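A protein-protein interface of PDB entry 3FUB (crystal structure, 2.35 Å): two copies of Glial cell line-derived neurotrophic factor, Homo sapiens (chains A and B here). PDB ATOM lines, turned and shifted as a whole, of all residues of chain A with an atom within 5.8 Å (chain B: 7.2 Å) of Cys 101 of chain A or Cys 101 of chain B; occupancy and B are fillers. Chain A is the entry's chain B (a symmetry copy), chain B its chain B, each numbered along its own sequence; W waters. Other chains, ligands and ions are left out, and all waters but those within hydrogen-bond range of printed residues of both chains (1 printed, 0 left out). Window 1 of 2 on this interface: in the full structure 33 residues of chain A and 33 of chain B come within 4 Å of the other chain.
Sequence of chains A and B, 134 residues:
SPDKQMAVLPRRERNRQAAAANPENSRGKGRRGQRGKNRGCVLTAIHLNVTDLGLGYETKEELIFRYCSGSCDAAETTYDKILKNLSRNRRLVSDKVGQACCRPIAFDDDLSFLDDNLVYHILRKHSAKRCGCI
Among the printed residues, merely in contact across the chains: Arg 103 of chain A with Ala 100 of chain B (3.5 Å), Ala 100 of chain A with Arg 103 of chain B (3.5 Å), Ile 134 of chain A with Ile 134 of chain B (3.7 Å), Gln 99 of chain A with Arg 103 of chain B (3.7 Å) and Arg 103 of chain A with Gln 99 of chain B (3.7 Å).
The side-chain sulfur (SG) of Cys 72 of chain B sits close to the backbone NH (N) of Cys 101 of chain B (3.7 Å).
The backbone NH of Ile 134 of chain A sits at hydrogen-bond distance from the backbone carbonyl oxygen of Cys 101 of chain A (3.1 Å).
The backbone carbonyl oxygen of Cys 101 of chain B lies within hydrogen-bond range of the backbone NH of Ile 134 of chain B.
The side-chain sulfur of Cys 131 of chain B forms a disulfide with the side-chain sulfur of Cys 68 of chain B, at 2.0 Å.
The backbone NH (N) of Arg 103 of chain A sits at hydrogen-bond distance from the backbone carbonyl oxygen (O) of Gly 132 of chain A, at 2.9 Å.
SG of Cys 41 of chain B forms a disulfide with SG of Cys 102 of chain B (2.0 Å).
Cys 101 of chain A touches one residue of chain B.
Printed residues of chain A within 4 Å of Asp 80 of chain B: Arg 103 (3.3 Å).
Of the printed residues of chain A, Gln 99 of chain B touches Arg 103 (3.7 Å).
Cys 101 of chain B touches just one residue of chain A: Cys 101.
Of the 9 printed residues of chain A, 5 touch a printed residue of chain B.
Printed residues of chain A that touch a printed residue of chain B: Gln 99, Ala 100, Cys 101, Arg 103 and Ile 134.
Printed residues of chain B that touch a printed residue of chain A: Asp 80, Gly 98, Gln 99, Ala 100, Cys 101, Arg 103 and Ile 134.
Hydrophobic or aromatic side chains of chain B that line the printed part of chain A: Ala 100 and Ile 134.
Among the printed residues, 10 pairs touch across the chains.
Among the printed residues, Asp or Glu carboxylates within 4 Å of a Lys or Arg side-chain nitrogen of the other chain: Arg 103 of chain A with Asp 80 of chain B (3.3 Å).
The chain-end carboxylate (OXT) of Ile 134 of chain B lies within salt-bridge range of the guanidinium group (NE) of Arg 103 of chain A, at 3.0 Å.
The side-chain carboxylate (OD2) of Asp 80 of chain B lies within salt-bridge range of the guanidinium group (NH2) of Arg 103 of chain A (3.3 Å).
The guanidinium group (NE) of Arg 103 of chain B is in salt-bridge range of the chain-end carboxylate (OXT) of Ile 134 of chain A (3.0 Å).
The side-chain sulfur of Cys 101 of chain B forms a disulfide with the side-chain sulfur of Cys 101 of chain A, at 2.0 Å.
The backbone carbonyl oxygen of Gly 98 of chain B sits at hydrogen-bond distance from the guanidinium group of Arg 103 of chain A (3.2 Å).
Gln 99 of chain A touches Arg 103 of chain B, and with the chains exchanged Arg 103 of chain A touches Gln 99 of chain B.
Cys 101 of chain A touches its own counterpart, Cys 101 of chain B.
Arg 103 of chain A touches Ile 134 of chain B, and with the chains exchanged Ile 134 of chain A touches Arg 103 of chain B.
Ile 134 of chain B touches its own counterpart, Ile 134 of chain A.
9 positions are printed for both chains.
Of the 10 pairs that touch across the chains among the printed residues, 8 have their exchanged pair printed and touching as well.
Water W1 lies within hydrogen-bond range of O of Gly 98 of chain B (3.0 Å) and O of Cys 102 of chain A (3.4 Å).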
ATOM      1  N   CYS A  72       2.865  21.806  28.503  1.00  0.00           N
ATOM      2  CA  CYS A  72       1.632  21.021  28.625  1.00  0.00           C
ATOM      3  C   CYS A  72       1.681  19.969  29.735  1.00  0.00           C
ATOM      4  O   CYS A  72       2.761  19.560  30.172  1.00  0.00           O
ATOM      5  CB  CYS A  72       1.260  20.378  27.284  1.00  0.00           C
ATOM      6  SG  CYS A  72       0.499  21.527  26.095  1.00  0.00           S
ATOM      7  N   GLN A  99       4.422  14.798  21.612  1.00  0.00           N
ATOM      8  CA  GLN A  99       3.397  15.322  22.528  1.00  0.00           C
ATOM      9  C   GLN A  99       2.658  16.605  22.130  1.00  0.00           C
ATOM     10  O   GLN A  99       2.929  17.206  21.089  1.00  0.00           O
ATOM     11  CB  GLN A  99       3.957  15.438  23.952  1.00  0.00           C
ATOM     12  CG  GLN A  99       4.206  14.087  24.622  1.00  0.00           C
ATOM     13  CD  GLN A  99       3.728  14.036  26.061  1.00  0.00           C
ATOM     14  OE1 GLN A  99       3.071  13.081  26.469  1.00  0.00           O
ATOM     15  NE2 GLN A  99       4.050  15.068  26.836  1.00  0.00           N
ATOM     16  N   ALA A 100       1.719  16.997  22.991  1.00  0.00           N
ATOM     17  CA  ALA A 100       0.806  18.110  22.753  1.00  0.00           C
ATOM     18  C   ALA A 100       1.482  19.468  22.901  1.00  0.00           C
ATOM     19  O   ALA A 100       2.621  19.561  23.365  1.00  0.00           O
ATOM     20  CB  ALA A 100      -0.389  18.008  23.690  1.00  0.00           C
ATOM     21  N   CYS A 101       0.768  20.518  22.495  1.00  0.00           N
ATOM     22  CA  CYS A 101       1.283  21.884  22.541  1.00  0.00           C
ATOM     23  C   CYS A 101       0.206  22.875  22.940  1.00  0.00           C
ATOM     24  O   CYS A 101      -0.948  22.742  22.538  1.00  0.00           O
ATOM     25  CB  CYS A 101       1.843  22.292  21.185  1.00  0.00           C
ATOM     26  SG  CYS A 101       2.804  21.007  20.363  1.00  0.00           S
ATOM     27  N   CYS A 102       0.605  23.867  23.731  1.00  0.00           N
ATOM     28  CA  CYS A 102      -0.260  24.979  24.100  1.00  0.00           C
ATOM     29  C   CYS A 102      -0.449  25.879  22.878  1.00  0.00           C
ATOM     30  O   CYS A 102       0.472  26.588  22.463  1.00  0.00           O
ATOM     31  CB  CYS A 102       0.342  25.750  25.271  1.00  0.00           C
ATOM     32  SG  CYS A 102      -0.629  27.157  25.815  1.00  0.00           S
ATOM     33  N   ARG A 103      -1.650  25.819  22.303  1.00  0.00           N
ATOM     34  CA  ARG A 103      -1.951  26.425  21.010  1.00  0.00           C
ATOM     35  C   ARG A 103      -3.299  27.151  21.056  1.00  0.00           C
ATOM     36  O   ARG A 103      -4.068  26.950  21.996  1.00  0.00           O
ATOM     37  CB  ARG A 103      -1.969  25.345  19.920  1.00  0.00           C
ATOM     38  CG  ARG A 103      -0.614  24.711  19.606  1.00  0.00           C
ATOM     39  CD  ARG A 103       0.310  25.685  18.889  1.00  0.00           C
ATOM     40  NE  ARG A 103      -0.022  25.824  17.471  1.00  0.00           N
ATOM     41  CZ  ARG A 103       0.290  26.880  16.723  1.00  0.00           C
ATOM     42  NH1 ARG A 103       0.938  27.915  17.251  1.00  0.00           N
ATOM     43  NH2 ARG A 103      -0.051  26.909  15.441  1.00  0.00           N
ATOM     44  N   GLY A 132      -5.474  26.015  24.521  1.00  0.00           N
ATOM     45  CA  GLY A 132      -5.522  24.695  25.136  1.00  0.00           C
ATOM     46  C   GLY A 132      -4.334  23.871  24.687  1.00  0.00           C
ATOM     47  O   GLY A 132      -3.626  24.248  23.747  1.00  0.00           O
ATOM     48  N   CYS A 133      -4.100  22.755  25.371  1.00  0.00           N
ATOM     49  CA  CYS A 133      -3.115  21.774  24.924  1.00  0.00           C
ATOM     50  C   CYS A 133      -3.792  20.784  23.985  1.00  0.00           C
ATOM     51  O   CYS A 133      -4.735  20.090  24.368  1.00  0.00           O
ATOM     52  CB  CYS A 133      -2.465  21.065  26.111  1.00  0.00           C
ATOM     53  SG  CYS A 133      -1.244  22.075  26.977  1.00  0.00           S
ATOM     54  N   ILE A 134      -3.311  20.744  22.747  1.00  0.00           N
ATOM     55  CA  ILE A 134      -3.963  19.994  21.679  1.00  0.00           C
ATOM     56  C   ILE A 134      -2.961  19.158  20.895  1.00  0.00           C
ATOM     57  O   ILE A 134      -1.764  19.442  20.896  1.00  0.00           O
ATOM     58  CB  ILE A 134      -4.695  20.938  20.694  1.00  0.00           C
ATOM     59  CG1 ILE A 134      -3.737  22.024  20.181  1.00  0.00           C
ATOM     60  CG2 ILE A 134      -5.935  21.550  21.360  1.00  0.00           C
ATOM     61  CD1 ILE A 134      -4.175  22.702  18.902  1.00  0.00           C
ATOM     62  OXT ILE A 134      -3.330  18.186  20.234  1.00  0.00           O
ATOM     63  N   CYS B  41       5.385  15.912   7.869  1.00  0.00           N
ATOM     64  CA  CYS B  41       4.434  15.504   8.899  1.00  0.00           C
ATOM     65  C   CYS B  41       3.565  14.362   8.368  1.00  0.00           C
ATOM     66  O   CYS B  41       2.634  14.585   7.584  1.00  0.00           O
ATOM     67  CB  CYS B  41       3.579  16.701   9.331  1.00  0.00           C
ATOM     68  SG  CYS B  41       2.064  16.303  10.243  1.00  0.00           S
ATOM     69  N   CYS B  68       1.318  10.471  14.624  1.00  0.00           N
ATOM     70  CA  CYS B  68       1.814  11.543  13.757  1.00  0.00           C
ATOM     71  C   CYS B  68       3.269  11.897  14.072  1.00  0.00           C
ATOM     72  O   CYS B  68       3.620  12.128  15.231  1.00  0.00           O
ATOM     73  CB  CYS B  68       0.941  12.788  13.910  1.00  0.00           C
ATOM     74  SG  CYS B  68      -0.824  12.483  13.718  1.00  0.00           S
ATOM     75  N   GLY B  70       7.137  13.970  12.586  1.00  0.00           N
ATOM     76  CA  GLY B  70       7.817  14.936  11.718  1.00  0.00           C
ATOM     77  C   GLY B  70       7.855  16.363  12.240  1.00  0.00           C
ATOM     78  O   GLY B  70       7.317  16.658  13.306  1.00  0.00           O
ATOM     79  N   SER B  71       8.502  17.247  11.481  1.00  0.00           N
ATOM     80  CA  SER B  71       8.536  18.677  11.794  1.00  0.00           C
ATOM     81  C   SER B  71       7.536  19.456  10.931  1.00  0.00           C
ATOM     82  O   SER B  71       7.053  18.947   9.914  1.00  0.00           O
ATOM     83  CB  SER B  71       9.951  19.235  11.615  1.00  0.00           C
ATOM     84  OG  SER B  71      10.078  20.511  12.219  1.00  0.00           O
ATOM     85  N   CYS B  72       7.234  20.689  11.337  1.00  0.00           N
ATOM     86  CA  CYS B  72       6.235  21.510  10.645  1.00  0.00           C
ATOM     87  C   CYS B  72       6.843  22.552   9.702  1.00  0.00           C
ATOM     88  O   CYS B  72       8.011  22.924   9.840  1.00  0.00           O
ATOM     89  CB  CYS B  72       5.286  22.176  11.648  1.00  0.00           C
ATOM     90  SG  CYS B  72       4.012  21.059  12.317  1.00  0.00           S
ATOM     91  N   ASP B  80       1.558  32.070  13.002  1.00  0.00           N
ATOM     92  CA  ASP B  80       2.926  31.548  13.086  1.00  0.00           C
ATOM     93  C   ASP B  80       3.919  32.471  12.394  1.00  0.00           C
ATOM     94  O   ASP B  80       5.066  32.620  12.844  1.00  0.00           O
ATOM     95  CB  ASP B  80       3.029  30.129  12.510  1.00  0.00           C
ATOM     96  CG  ASP B  80       2.447  29.074  13.443  1.00  0.00           C
ATOM     97  OD1 ASP B  80       2.769  29.092  14.650  1.00  0.00           O
ATOM     98  OD2 ASP B  80       1.663  28.224  12.965  1.00  0.00           O
ATOM     99  N   VAL B  97       8.311  29.330  23.769  1.00  0.00           N
ATOM    100  CA  VAL B  97       6.982  28.776  23.491  1.00  0.00           C
ATOM    101  C   VAL B  97       6.382  29.457  22.256  1.00  0.00           C
ATOM    102  O   VAL B  97       6.332  30.692  22.182  1.00  0.00           O
ATOM    103  CB  VAL B  97       5.985  28.944  24.673  1.00  0.00           C
ATOM    104  CG1 VAL B  97       4.861  27.926  24.541  1.00  0.00           C
ATOM    105  CG2 VAL B  97       6.674  28.807  26.031  1.00  0.00           C
ATOM    106  N   GLY B  98       5.920  28.655  21.296  1.00  0.00           N
ATOM    107  CA  GLY B  98       5.356  29.207  20.071  1.00  0.00           C
ATOM    108  C   GLY B  98       4.696  28.270  19.074  1.00  0.00           C
ATOM    109  O   GLY B  98       3.480  28.067  19.113  1.00  0.00           O
ATOM    110  N   GLN B  99       5.508  27.700  18.186  1.00  0.00           N
ATOM    111  CA  GLN B  99       5.033  27.200  16.885  1.00  0.00           C
ATOM    112  C   GLN B  99       4.155  25.944  16.870  1.00  0.00           C
ATOM    113  O   GLN B  99       3.875  25.343  17.908  1.00  0.00           O
ATOM    114  CB  GLN B  99       6.203  27.056  15.903  1.00  0.00           C
ATOM    115  CG  GLN B  99       6.784  28.394  15.446  1.00  0.00           C
ATOM    116  CD  GLN B  99       7.057  28.448  13.954  1.00  0.00           C
ATOM    117  OE1 GLN B  99       6.705  29.419  13.289  1.00  0.00           O
ATOM    118  NE2 GLN B  99       7.679  27.401  13.421  1.00  0.00           N
ATOM    119  N   ALA B 100       3.732  25.574  15.662  1.00  0.00           N
ATOM    120  CA  ALA B 100       2.783  24.491  15.424  1.00  0.00           C
ATOM    121  C   ALA B 100       3.405  23.112  15.608  1.00  0.00           C
ATOM    122  O   ALA B 100       4.624  22.981  15.745  1.00  0.00           O
ATOM    123  CB  ALA B 100       2.188  24.623  14.029  1.00  0.00           C
ATOM    124  N   CYS B 101       2.552  22.087  15.612  1.00  0.00           N
ATOM    125  CA  CYS B 101       2.984  20.706  15.808  1.00  0.00           C
ATOM    126  C   CYS B 101       2.201  19.746  14.935  1.00  0.00           C
ATOM    127  O   CYS B 101       1.000  19.917  14.735  1.00  0.00           O
ATOM    128  CB  CYS B 101       2.812  20.292  17.264  1.00  0.00           C
ATOM    129  SG  CYS B 101       3.300  21.553  18.456  1.00  0.00           S
ATOM    130  N   CYS B 102       2.899  18.735  14.424  1.00  0.00           N
ATOM    131  CA  CYS B 102       2.284  17.647  13.676  1.00  0.00           C
ATOM    132  C   CYS B 102       1.504  16.764  14.651  1.00  0.00           C
ATOM    133  O   CYS B 102       2.092  16.030  15.451  1.00  0.00           O
ATOM    134  CB  CYS B 102       3.350  16.850  12.932  1.00  0.00           C
ATOM    135  SG  CYS B 102       2.717  15.469  11.978  1.00  0.00           S
ATOM    136  N   ARG B 103       0.177  16.865  14.580  1.00  0.00           N
ATOM    137  CA  ARG B 103      -0.725  16.279  15.566  1.00  0.00           C
ATOM    138  C   ARG B 103      -1.908  15.594  14.873  1.00  0.00           C
ATOM    139  O   ARG B 103      -2.125  15.811  13.681  1.00  0.00           O
ATOM    140  CB  ARG B 103      -1.231  17.367  16.522  1.00  0.00           C
ATOM    141  CG  ARG B 103      -0.174  17.961  17.452  1.00  0.00           C
ATOM    142  CD  ARG B 103       0.263  16.965  18.517  1.00  0.00           C
ATOM    143  NE  ARG B 103      -0.713  16.848  19.600  1.00  0.00           N
ATOM    144  CZ  ARG B 103      -0.830  15.789  20.399  1.00  0.00           C
ATOM    145  NH1 ARG B 103      -0.040  14.731  20.238  1.00  0.00           N
ATOM    146  NH2 ARG B 103      -1.744  15.780  21.359  1.00  0.00           N
ATOM    147  N   PRO B 104      -2.668  14.754  15.610  1.00  0.00           N
ATOM    148  CA  PRO B 104      -3.821  14.082  15.004  1.00  0.00           C
ATOM    149  C   PRO B 104      -4.957  15.054  14.723  1.00  0.00           C
ATOM    150  O   PRO B 104      -5.318  15.840  15.596  1.00  0.00           O
ATOM    151  CB  PRO B 104      -4.261  13.079  16.082  1.00  0.00           C
ATOM    152  CG  PRO B 104      -3.137  12.995  17.029  1.00  0.00           C
ATOM    153  CD  PRO B 104      -2.472  14.324  17.005  1.00  0.00           C
ATOM    154  N   CYS B 131      -3.242  13.437  10.109  1.00  0.00           N
ATOM    155  CA  CYS B 131      -2.348  14.363  10.791  1.00  0.00           C
ATOM    156  C   CYS B 131      -2.204  15.682  10.041  1.00  0.00           C
ATOM    157  O   CYS B 131      -2.176  15.715   8.810  1.00  0.00           O
ATOM    158  CB  CYS B 131      -0.970  13.728  10.981  1.00  0.00           C
ATOM    159  SG  CYS B 131      -1.007  12.097  11.739  1.00  0.00           S
ATOM    160  N   GLY B 132      -2.118  16.769  10.798  1.00  0.00           N
ATOM    161  CA  GLY B 132      -1.825  18.085  10.246  1.00  0.00           C
ATOM    162  C   GLY B 132      -0.973  18.875  11.216  1.00  0.00           C
ATOM    163  O   GLY B 132      -0.815  18.484  12.378  1.00  0.00           O
ATOM    164  N   CYS B 133      -0.405  19.978  10.737  1.00  0.00           N
ATOM    165  CA  CYS B 133       0.274  20.932  11.609  1.00  0.00           C
ATOM    166  C   CYS B 133      -0.740  21.950  12.116  1.00  0.00           C
ATOM    167  O   CYS B 133      -1.363  22.670  11.334  1.00  0.00           O
ATOM    168  CB  CYS B 133       1.435  21.612  10.885  1.00  0.00           C
ATOM    169  SG  CYS B 133       2.890  20.558  10.703  1.00  0.00           S
ATOM    170  N   ILE B 134      -0.911  21.985  13.433  1.00  0.00           N
ATOM    171  CA  ILE B 134      -1.972  22.763  14.064  1.00  0.00           C
ATOM    172  C   ILE B 134      -1.444  23.574  15.238  1.00  0.00           C
ATOM    173  O   ILE B 134      -0.402  23.253  15.810  1.00  0.00           O
ATOM    174  CB  ILE B 134      -3.115  21.849  14.569  1.00  0.00           C
ATOM    175  CG1 ILE B 134      -2.555  20.738  15.471  1.00  0.00           C
ATOM    176  CG2 ILE B 134      -3.902  21.271  13.385  1.00  0.00           C
ATOM    177  CD1 ILE B 134      -3.572  20.084  16.377  1.00  0.00           C
ATOM    178  OXT ILE B 134      -2.055  24.562  15.650  1.00  0.00           O
HETATM  179  O   HOH W   1       1.530  29.375  20.907  1.00  0.00           O
